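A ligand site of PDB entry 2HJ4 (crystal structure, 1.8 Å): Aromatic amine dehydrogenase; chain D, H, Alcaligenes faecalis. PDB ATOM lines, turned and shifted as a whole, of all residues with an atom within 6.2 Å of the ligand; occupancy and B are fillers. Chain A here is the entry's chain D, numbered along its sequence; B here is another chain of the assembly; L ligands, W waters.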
ATOM      1  N   ASP A  37      19.877  25.528 -12.752  1.00  0.00           N
ATOM      2  CA  ASP A  37      20.158  26.765 -13.434  1.00  0.00           C
ATOM      3  C   ASP A  37      18.913  27.031 -14.248  1.00  0.00           C
ATOM      4  O   ASP A  37      18.744  26.478 -15.337  1.00  0.00           O
ATOM      5  CB  ASP A  37      21.440  26.685 -14.282  1.00  0.00           C
ATOM      6  CG  ASP A  37      21.974  28.085 -14.661  1.00  0.00           C
ATOM      7  OD1 ASP A  37      21.310  29.110 -14.360  1.00  0.00           O
ATOM      8  OD2 ASP A  37      23.066  28.155 -15.250  1.00  0.00           O
ATOM      9  N   GLY A  38      17.997  27.799 -13.658  1.00  0.00           N
ATOM     10  CA  GLY A  38      16.714  28.127 -14.280  1.00  0.00           C
ATOM     11  C   GLY A  38      15.761  28.749 -13.300  1.00  0.00           C
ATOM     12  O   GLY A  38      16.143  29.164 -12.205  1.00  0.00           O
ATOM     13  N   TRQ A  62      19.053  16.559 -16.615  1.00  0.00           N
ATOM     14  CA  TRQ A  62      20.290  16.387 -15.873  1.00  0.00           C
ATOM     15  C   TRQ A  62      19.919  16.098 -14.418  1.00  0.00           C
ATOM     16  O   TRQ A  62      18.798  16.388 -13.968  1.00  0.00           O
ATOM     17  CB  TRQ A  62      21.208  17.598 -15.956  1.00  0.00           C
ATOM     18  CG  TRQ A  62      20.707  18.824 -15.290  1.00  0.00           C
ATOM     19  CD1 TRQ A  62      20.969  19.164 -14.009  1.00  0.00           C
ATOM     20  NE1 TRQ A  62      20.361  20.337 -13.697  1.00  0.00           N
ATOM     21  CE2 TRQ A  62      19.691  20.802 -14.792  1.00  0.00           C
ATOM     22  CZ2 TRQ A  62      18.943  21.954 -14.935  1.00  0.00           C
ATOM     23  CH2 TRQ A  62      18.347  22.213 -16.131  1.00  0.00           C
ATOM     24  CZ3 TRQ A  62      18.499  21.334 -17.222  1.00  0.00           C
ATOM     25  CE3 TRQ A  62      19.283  20.121 -17.072  1.00  0.00           C
ATOM     26  CD2 TRQ A  62      19.886  19.875 -15.827  1.00  0.00           C
ATOM     27  O6  TRQ A  62      17.610  23.334 -16.223  1.00  0.00           O
ATOM     28  O7  TRQ A  62      18.849  22.752 -13.881  1.00  0.00           O
ATOM     29  N   ASP A  81      12.535  19.605 -16.517  1.00  0.00           N
ATOM     30  CA  ASP A  81      12.039  20.922 -16.842  1.00  0.00           C
ATOM     31  C   ASP A  81      10.583  20.821 -17.158  1.00  0.00           C
ATOM     32  O   ASP A  81      10.065  19.725 -17.401  1.00  0.00           O
ATOM     33  CB  ASP A  81      12.793  21.475 -18.059  1.00  0.00           C
ATOM     34  CG  ASP A  81      14.175  21.913 -17.717  1.00  0.00           C
ATOM     35  OD1 ASP A  81      14.404  22.276 -16.543  1.00  0.00           O
ATOM     36  OD2 ASP A  81      15.059  21.929 -18.606  1.00  0.00           O
ATOM     37  N   ASN A 109      24.184  21.297 -16.809  1.00  0.00           N
ATOM     38  CA  ASN A 109      23.020  22.185 -16.803  1.00  0.00           C
ATOM     39  C   ASN A 109      23.104  23.460 -17.663  1.00  0.00           C
ATOM     40  O   ASN A 109      22.261  24.335 -17.519  1.00  0.00           O
ATOM     41  CB  ASN A 109      22.567  22.523 -15.347  1.00  0.00           C
ATOM     42  CG  ASN A 109      23.491  23.509 -14.598  1.00  0.00           C
ATOM     43  OD1 ASN A 109      24.371  24.143 -15.166  1.00  0.00           O
ATOM     44  ND2 ASN A 109      23.260  23.653 -13.286  1.00  0.00           N
ATOM     45  N   ASP A 110      24.067  23.537 -18.587  1.00  0.00           N
ATOM     46  CA  ASP A 110      24.145  24.689 -19.504  1.00  0.00           C
ATOM     47  C   ASP A 110      23.473  24.405 -20.831  1.00  0.00           C
ATOM     48  O   ASP A 110      23.617  25.193 -21.785  1.00  0.00           O
ATOM     49  CB  ASP A 110      25.586  25.088 -19.777  1.00  0.00           C
ATOM     50  CG  ASP A 110      26.314  25.610 -18.547  1.00  0.00           C
ATOM     51  OD1 ASP A 110      25.659  26.095 -17.578  1.00  0.00           O
ATOM     52  OD2 ASP A 110      27.547  25.515 -18.546  1.00  0.00           O
ATOM     53  N   VAL A 111      22.727  23.323 -20.880  1.00  0.00           N
ATOM     54  CA  VAL A 111      21.913  22.968 -22.014  1.00  0.00           C
ATOM     55  C   VAL A 111      20.440  22.938 -21.574  1.00  0.00           C
ATOM     56  O   VAL A 111      20.120  22.856 -20.380  1.00  0.00           O
ATOM     57  CB  VAL A 111      22.295  21.581 -22.611  1.00  0.00           C
ATOM     58  CG1 VAL A 111      23.661  21.634 -23.221  1.00  0.00           C
ATOM     59  CG2 VAL A 111      22.221  20.467 -21.552  1.00  0.00           C
ATOM     60  N   ASN A 112      19.568  23.004 -22.560  1.00  0.00           N
ATOM     61  CA  ASN A 112      18.143  23.030 -22.353  1.00  0.00           C
ATOM     62  C   ASN A 112      17.577  21.611 -22.188  1.00  0.00           C
ATOM     63  O   ASN A 112      17.441  20.903 -23.172  1.00  0.00           O
ATOM     64  CB  ASN A 112      17.482  23.678 -23.564  1.00  0.00           C
ATOM     65  CG  ASN A 112      15.985  23.846 -23.379  1.00  0.00           C
ATOM     66  OD1 ASN A 112      15.488  23.819 -22.254  1.00  0.00           O
ATOM     67  ND2 ASN A 112      15.259  24.031 -24.485  1.00  0.00           N
ATOM     68  N   TRP A 113      17.240  21.192 -20.990  1.00  0.00           N
ATOM     69  CA  TRP A 113      16.656  19.839 -20.841  1.00  0.00           C
ATOM     70  C   TRP A 113      15.204  19.658 -21.364  1.00  0.00           C
ATOM     71  O   TRP A 113      14.653  18.554 -21.329  1.00  0.00           O
ATOM     72  CB  TRP A 113      16.883  19.264 -19.408  1.00  0.00           C
ATOM     73  CG  TRP A 113      18.314  18.848 -19.270  1.00  0.00           C
ATOM     74  CD1 TRP A 113      19.270  19.375 -18.449  1.00  0.00           C
ATOM     75  CD2 TRP A 113      18.948  17.847 -20.054  1.00  0.00           C
ATOM     76  NE1 TRP A 113      20.480  18.749 -18.710  1.00  0.00           N
ATOM     77  CE2 TRP A 113      20.297  17.802 -19.678  1.00  0.00           C
ATOM     78  CE3 TRP A 113      18.498  16.960 -21.028  1.00  0.00           C
ATOM     79  CZ2 TRP A 113      21.196  16.901 -20.230  1.00  0.00           C
ATOM     80  CZ3 TRP A 113      19.385  16.086 -21.585  1.00  0.00           C
ATOM     81  CH2 TRP A 113      20.715  16.060 -21.187  1.00  0.00           C
ATOM     82  N   PHE A 122      11.776  26.700 -23.092  1.00  0.00           N
ATOM     83  CA  PHE A 122      12.029  26.466 -21.667  1.00  0.00           C
ATOM     84  C   PHE A 122      11.182  27.361 -20.777  1.00  0.00           C
ATOM     85  O   PHE A 122      11.256  28.577 -20.886  1.00  0.00           O
ATOM     86  CB  PHE A 122      13.503  26.667 -21.335  1.00  0.00           C
ATOM     87  CG  PHE A 122      13.795  26.658 -19.852  1.00  0.00           C
ATOM     88  CD1 PHE A 122      13.682  25.490 -19.127  1.00  0.00           C
ATOM     89  CD2 PHE A 122      14.136  27.819 -19.184  1.00  0.00           C
ATOM     90  CE1 PHE A 122      13.915  25.483 -17.747  1.00  0.00           C
ATOM     91  CE2 PHE A 122      14.373  27.809 -17.825  1.00  0.00           C
ATOM     92  CZ  PHE A 122      14.268  26.644 -17.104  1.00  0.00           C
ATOM     93  N   THR A 125      11.998  24.887 -14.060  1.00  0.00           N
ATOM     94  CA  THR A 125      12.756  23.681 -13.683  1.00  0.00           C
ATOM     95  C   THR A 125      12.158  23.131 -12.398  1.00  0.00           C
ATOM     96  O   THR A 125      11.841  23.909 -11.472  1.00  0.00           O
ATOM     97  CB  THR A 125      14.273  23.994 -13.446  1.00  0.00           C
ATOM     98  OG1 THR A 125      14.843  24.594 -14.626  1.00  0.00           O
ATOM     99  CG2 THR A 125      15.055  22.731 -13.135  1.00  0.00           C
ATOM    100  N   PHE B  25      18.132  35.615 -21.904  1.00  0.00           N
ATOM    101  CA  PHE B  25      17.597  34.426 -21.262  1.00  0.00           C
ATOM    102  C   PHE B  25      16.216  34.635 -20.632  1.00  0.00           C
ATOM    103  O   PHE B  25      15.383  33.736 -20.679  1.00  0.00           O
ATOM    104  CB  PHE B  25      18.587  33.928 -20.199  1.00  0.00           C
ATOM    105  CG  PHE B  25      18.242  32.586 -19.637  1.00  0.00           C
ATOM    106  CD1 PHE B  25      18.421  31.436 -20.396  1.00  0.00           C
ATOM    107  CD2 PHE B  25      17.742  32.455 -18.345  1.00  0.00           C
ATOM    108  CE1 PHE B  25      18.089  30.170 -19.875  1.00  0.00           C
ATOM    109  CE2 PHE B  25      17.434  31.190 -17.821  1.00  0.00           C
ATOM    110  CZ  PHE B  25      17.598  30.064 -18.594  1.00  0.00           C
ATOM    111  N   LEU B  28      14.121  34.255 -23.887  1.00  0.00           N
ATOM    112  CA  LEU B  28      15.059  33.522 -24.706  1.00  0.00           C
ATOM    113  C   LEU B  28      14.604  33.315 -26.130  1.00  0.00           C
ATOM    114  O   LEU B  28      15.381  32.939 -26.977  1.00  0.00           O
ATOM    115  CB  LEU B  28      15.313  32.174 -24.024  1.00  0.00           C
ATOM    116  CG  LEU B  28      16.383  31.227 -24.564  1.00  0.00           C
ATOM    117  CD1 LEU B  28      17.689  31.933 -24.770  1.00  0.00           C
ATOM    118  CD2 LEU B  28      16.494  30.048 -23.580  1.00  0.00           C
ATOM    119  N   PHE B  51      15.084  31.688 -30.810  1.00  0.00           N
ATOM    120  CA  PHE B  51      15.297  31.013 -29.537  1.00  0.00           C
ATOM    121  C   PHE B  51      16.742  30.534 -29.417  1.00  0.00           C
ATOM    122  O   PHE B  51      17.177  29.719 -30.216  1.00  0.00           O
ATOM    123  CB  PHE B  51      14.389  29.799 -29.435  1.00  0.00           C
ATOM    124  CG  PHE B  51      14.522  29.047 -28.144  1.00  0.00           C
ATOM    125  CD1 PHE B  51      13.948  29.545 -26.985  1.00  0.00           C
ATOM    126  CD2 PHE B  51      15.235  27.853 -28.086  1.00  0.00           C
ATOM    127  CE1 PHE B  51      14.028  28.812 -25.771  1.00  0.00           C
ATOM    128  CE2 PHE B  51      15.346  27.142 -26.890  1.00  0.00           C
ATOM    129  CZ  PHE B  51      14.739  27.625 -25.737  1.00  0.00           C
ATOM    130  N   ASN B  52      17.426  31.031 -28.407  1.00  0.00           N
ATOM    131  CA  ASN B  52      18.798  30.617 -28.117  1.00  0.00           C
ATOM    132  C   ASN B  52      19.649  30.561 -29.391  1.00  0.00           C
ATOM    133  O   ASN B  52      20.134  29.510 -29.777  1.00  0.00           O
ATOM    134  CB  ASN B  52      18.830  29.244 -27.408  1.00  0.00           C
ATOM    135  CG  ASN B  52      20.264  28.734 -27.186  1.00  0.00           C
ATOM    136  OD1 ASN B  52      20.588  27.598 -27.535  1.00  0.00           O
ATOM    137  ND2 ASN B  52      21.152  29.598 -26.661  1.00  0.00           N
ATOM    138  N   HIS B  54      22.914  31.034 -31.770  1.00  0.00           N
ATOM    139  CA  HIS B  54      24.369  30.975 -31.734  1.00  0.00           C
ATOM    140  C   HIS B  54      24.889  31.696 -32.981  1.00  0.00           C
ATOM    141  O   HIS B  54      24.160  31.808 -33.997  1.00  0.00           O
ATOM    142  CB  HIS B  54      24.841  29.513 -31.730  1.00  0.00           C
ATOM    143  CG  HIS B  54      24.468  28.792 -30.465  1.00  0.00           C
ATOM    144  ND1 HIS B  54      25.417  28.239 -29.613  1.00  0.00           N
ATOM    145  CD2 HIS B  54      23.269  28.526 -29.909  1.00  0.00           C
ATOM    146  CE1 HIS B  54      24.807  27.694 -28.580  1.00  0.00           C
ATOM    147  NE2 HIS B  54      23.498  27.839 -28.738  1.00  0.00           N
ATOM    148  N   GLN B 105      20.753  23.168 -27.825  1.00  0.00           N
ATOM    149  CA  GLN B 105      20.176  24.368 -27.246  1.00  0.00           C
ATOM    150  C   GLN B 105      20.863  24.516 -25.914  1.00  0.00           C
ATOM    151  O   GLN B 105      20.716  23.669 -25.038  1.00  0.00           O
ATOM    152  CB  GLN B 105      18.669  24.202 -27.114  1.00  0.00           C
ATOM    153  CG  GLN B 105      17.954  24.067 -28.496  1.00  0.00           C
ATOM    154  CD  GLN B 105      16.452  23.830 -28.410  1.00  0.00           C
ATOM    155  OE1 GLN B 105      15.692  24.031 -29.400  1.00  0.00           O
ATOM    156  NE2 GLN B 105      15.999  23.411 -27.238  1.00  0.00           N
ATOM    157  N   GLY B 106      21.645  25.574 -25.780  1.00  0.00           N
ATOM    158  CA  GLY B 106      22.456  25.783 -24.586  1.00  0.00           C
ATOM    159  C   GLY B 106      23.252  27.066 -24.652  1.00  0.00           C
ATOM    160  O   GLY B 106      23.299  27.764 -25.688  1.00  0.00           O
ATOM    161  N   LEU B 107      23.908  27.381 -23.540  1.00  0.00           N
ATOM    162  CA  LEU B 107      24.686  28.614 -23.406  1.00  0.00           C
ATOM    163  C   LEU B 107      25.786  28.662 -24.455  1.00  0.00           C
ATOM    164  O   LEU B 107      26.244  27.606 -24.930  1.00  0.00           O
ATOM    165  CB  LEU B 107      25.253  28.713 -21.996  1.00  0.00           C
ATOM    166  CG  LEU B 107      24.219  28.700 -20.849  1.00  0.00           C
ATOM    167  CD1 LEU B 107      24.972  28.881 -19.550  1.00  0.00           C
ATOM    168  CD2 LEU B 107      23.139  29.768 -21.028  1.00  0.00           C
HETATM  169  C1  LIG L   1      19.122  27.110 -22.534  1.00  0.00           C
HETATM  170  C2  LIG L   1      17.906  26.669 -22.048  1.00  0.00           C
HETATM  171  C3  LIG L   1      17.844  26.262 -20.460  1.00  0.00           C
HETATM  172  C4  LIG L   1      19.006  26.379 -19.709  1.00  0.00           C
HETATM  173  C5  LIG L   1      20.193  26.827 -20.331  1.00  0.00           C
HETATM  174  C6  LIG L   1      20.257  27.187 -21.694  1.00  0.00           C
HETATM  175  N1  LIG L   1      19.220  24.550 -17.909  1.00  0.00           N
HETATM  176  C7  LIG L   1      18.995  25.967 -18.270  1.00  0.00           C
HETATM  177  N2  LIG L   1      19.189  27.424 -23.850  1.00  0.00           N
HETATM  178  O1  LIG L   1      18.194  27.294 -24.521  1.00  0.00           O
HETATM  179  O2  LIG L   1      20.232  27.840 -24.303  1.00  0.00           O
HETATM  180  O   HOH W   1      20.361  28.958 -17.755  1.00  0.00           O
HETATM  181  O   HOH W   2      16.710  23.713 -19.298  1.00  0.00           O
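N1 of the ligand is in hydrogen-bond range of O6 of TRQ 62 (2.6 Å). A nitrogen (N1) of the ligand lies close to the backbone carbonyl oxygen (O) of Asp 37 (3.2 Å). ND2 of Asn 52 of chain B sits close to O2 of the ligand, 3.1 Å away. The backbone NH (N) of Gly 106 of chain B lies close to an oxygen (O2) of the ligand, at 3.1 Å. The backbone carbonyl oxygen of Asn 109 is in hydrogen-bond range of a nitrogen (N1) of the ligand, 3.1 Å away. O of Val 111 sits at hydrogen-bond distance from N1 of the ligand (3.1 Å).
The aromatic ring (CD1) of Trp 113 is bonded to CE3 of TRQ 62 (1.6 Å). The side-chain hydroxyl (OG1) of Thr 125 is in hydrogen-bond range of O6 of TRQ 62 (3.4 Å). The backbone carbonyl oxygen (O) of Leu 28 of chain B lies within hydrogen-bond range of the backbone NH (N) of Asn 52 of chain B (3.1 Å). OD1 of Asn 52 of chain B lies within hydrogen-bond range of NE2 of His 54 of chain B (3.2 Å). O of Gly 106 of chain B is in hydrogen-bond range of NE2 of His 54 of chain B (3.1 Å). The side-chain carboxylate of Asp 110 lies close to the side-chain amide oxygen of Asn 109, at 3.4 Å. The backbone NH of Asn 112 is in hydrogen-bond range of the backbone carbonyl oxygen of Gln 105 of chain B. The backbone NH of Leu 107 of chain B sits at hydrogen-bond distance from the backbone carbonyl oxygen of Asp 110 (2.8 Å).
O of Asp 110 touches C6 of the ligand (3.9 Å). CB of Asn 112 touches C2 of the ligand, at 3.4 Å. Phe 25 of chain B touches the ligand (CE1 to C4, 3.9 Å). Leu 28 of chain B touches the ligand. CZ of Phe 51 of chain B touches O1 of the ligand (3.7 Å). C of Gln 105 of chain B touches O2 of the ligand, at 3.7 Å. N of Leu 107 of chain B touches O2 of the ligand, 3.8 Å away. Within 4 Å of the ligand: Asp 37, TRQ 62, Asn 109, Asp 110, Val 111, Asn 112, Phe 25 of chain B, Leu 28 of chain B, Phe 51 of chain B, Asn 52 of chain B, Gln 105 of chain B, Gly 106 of chain B and Leu 107 of chain B. The nearest printed residue that does not touch the ligand is Phe 122 (4.1 Å).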
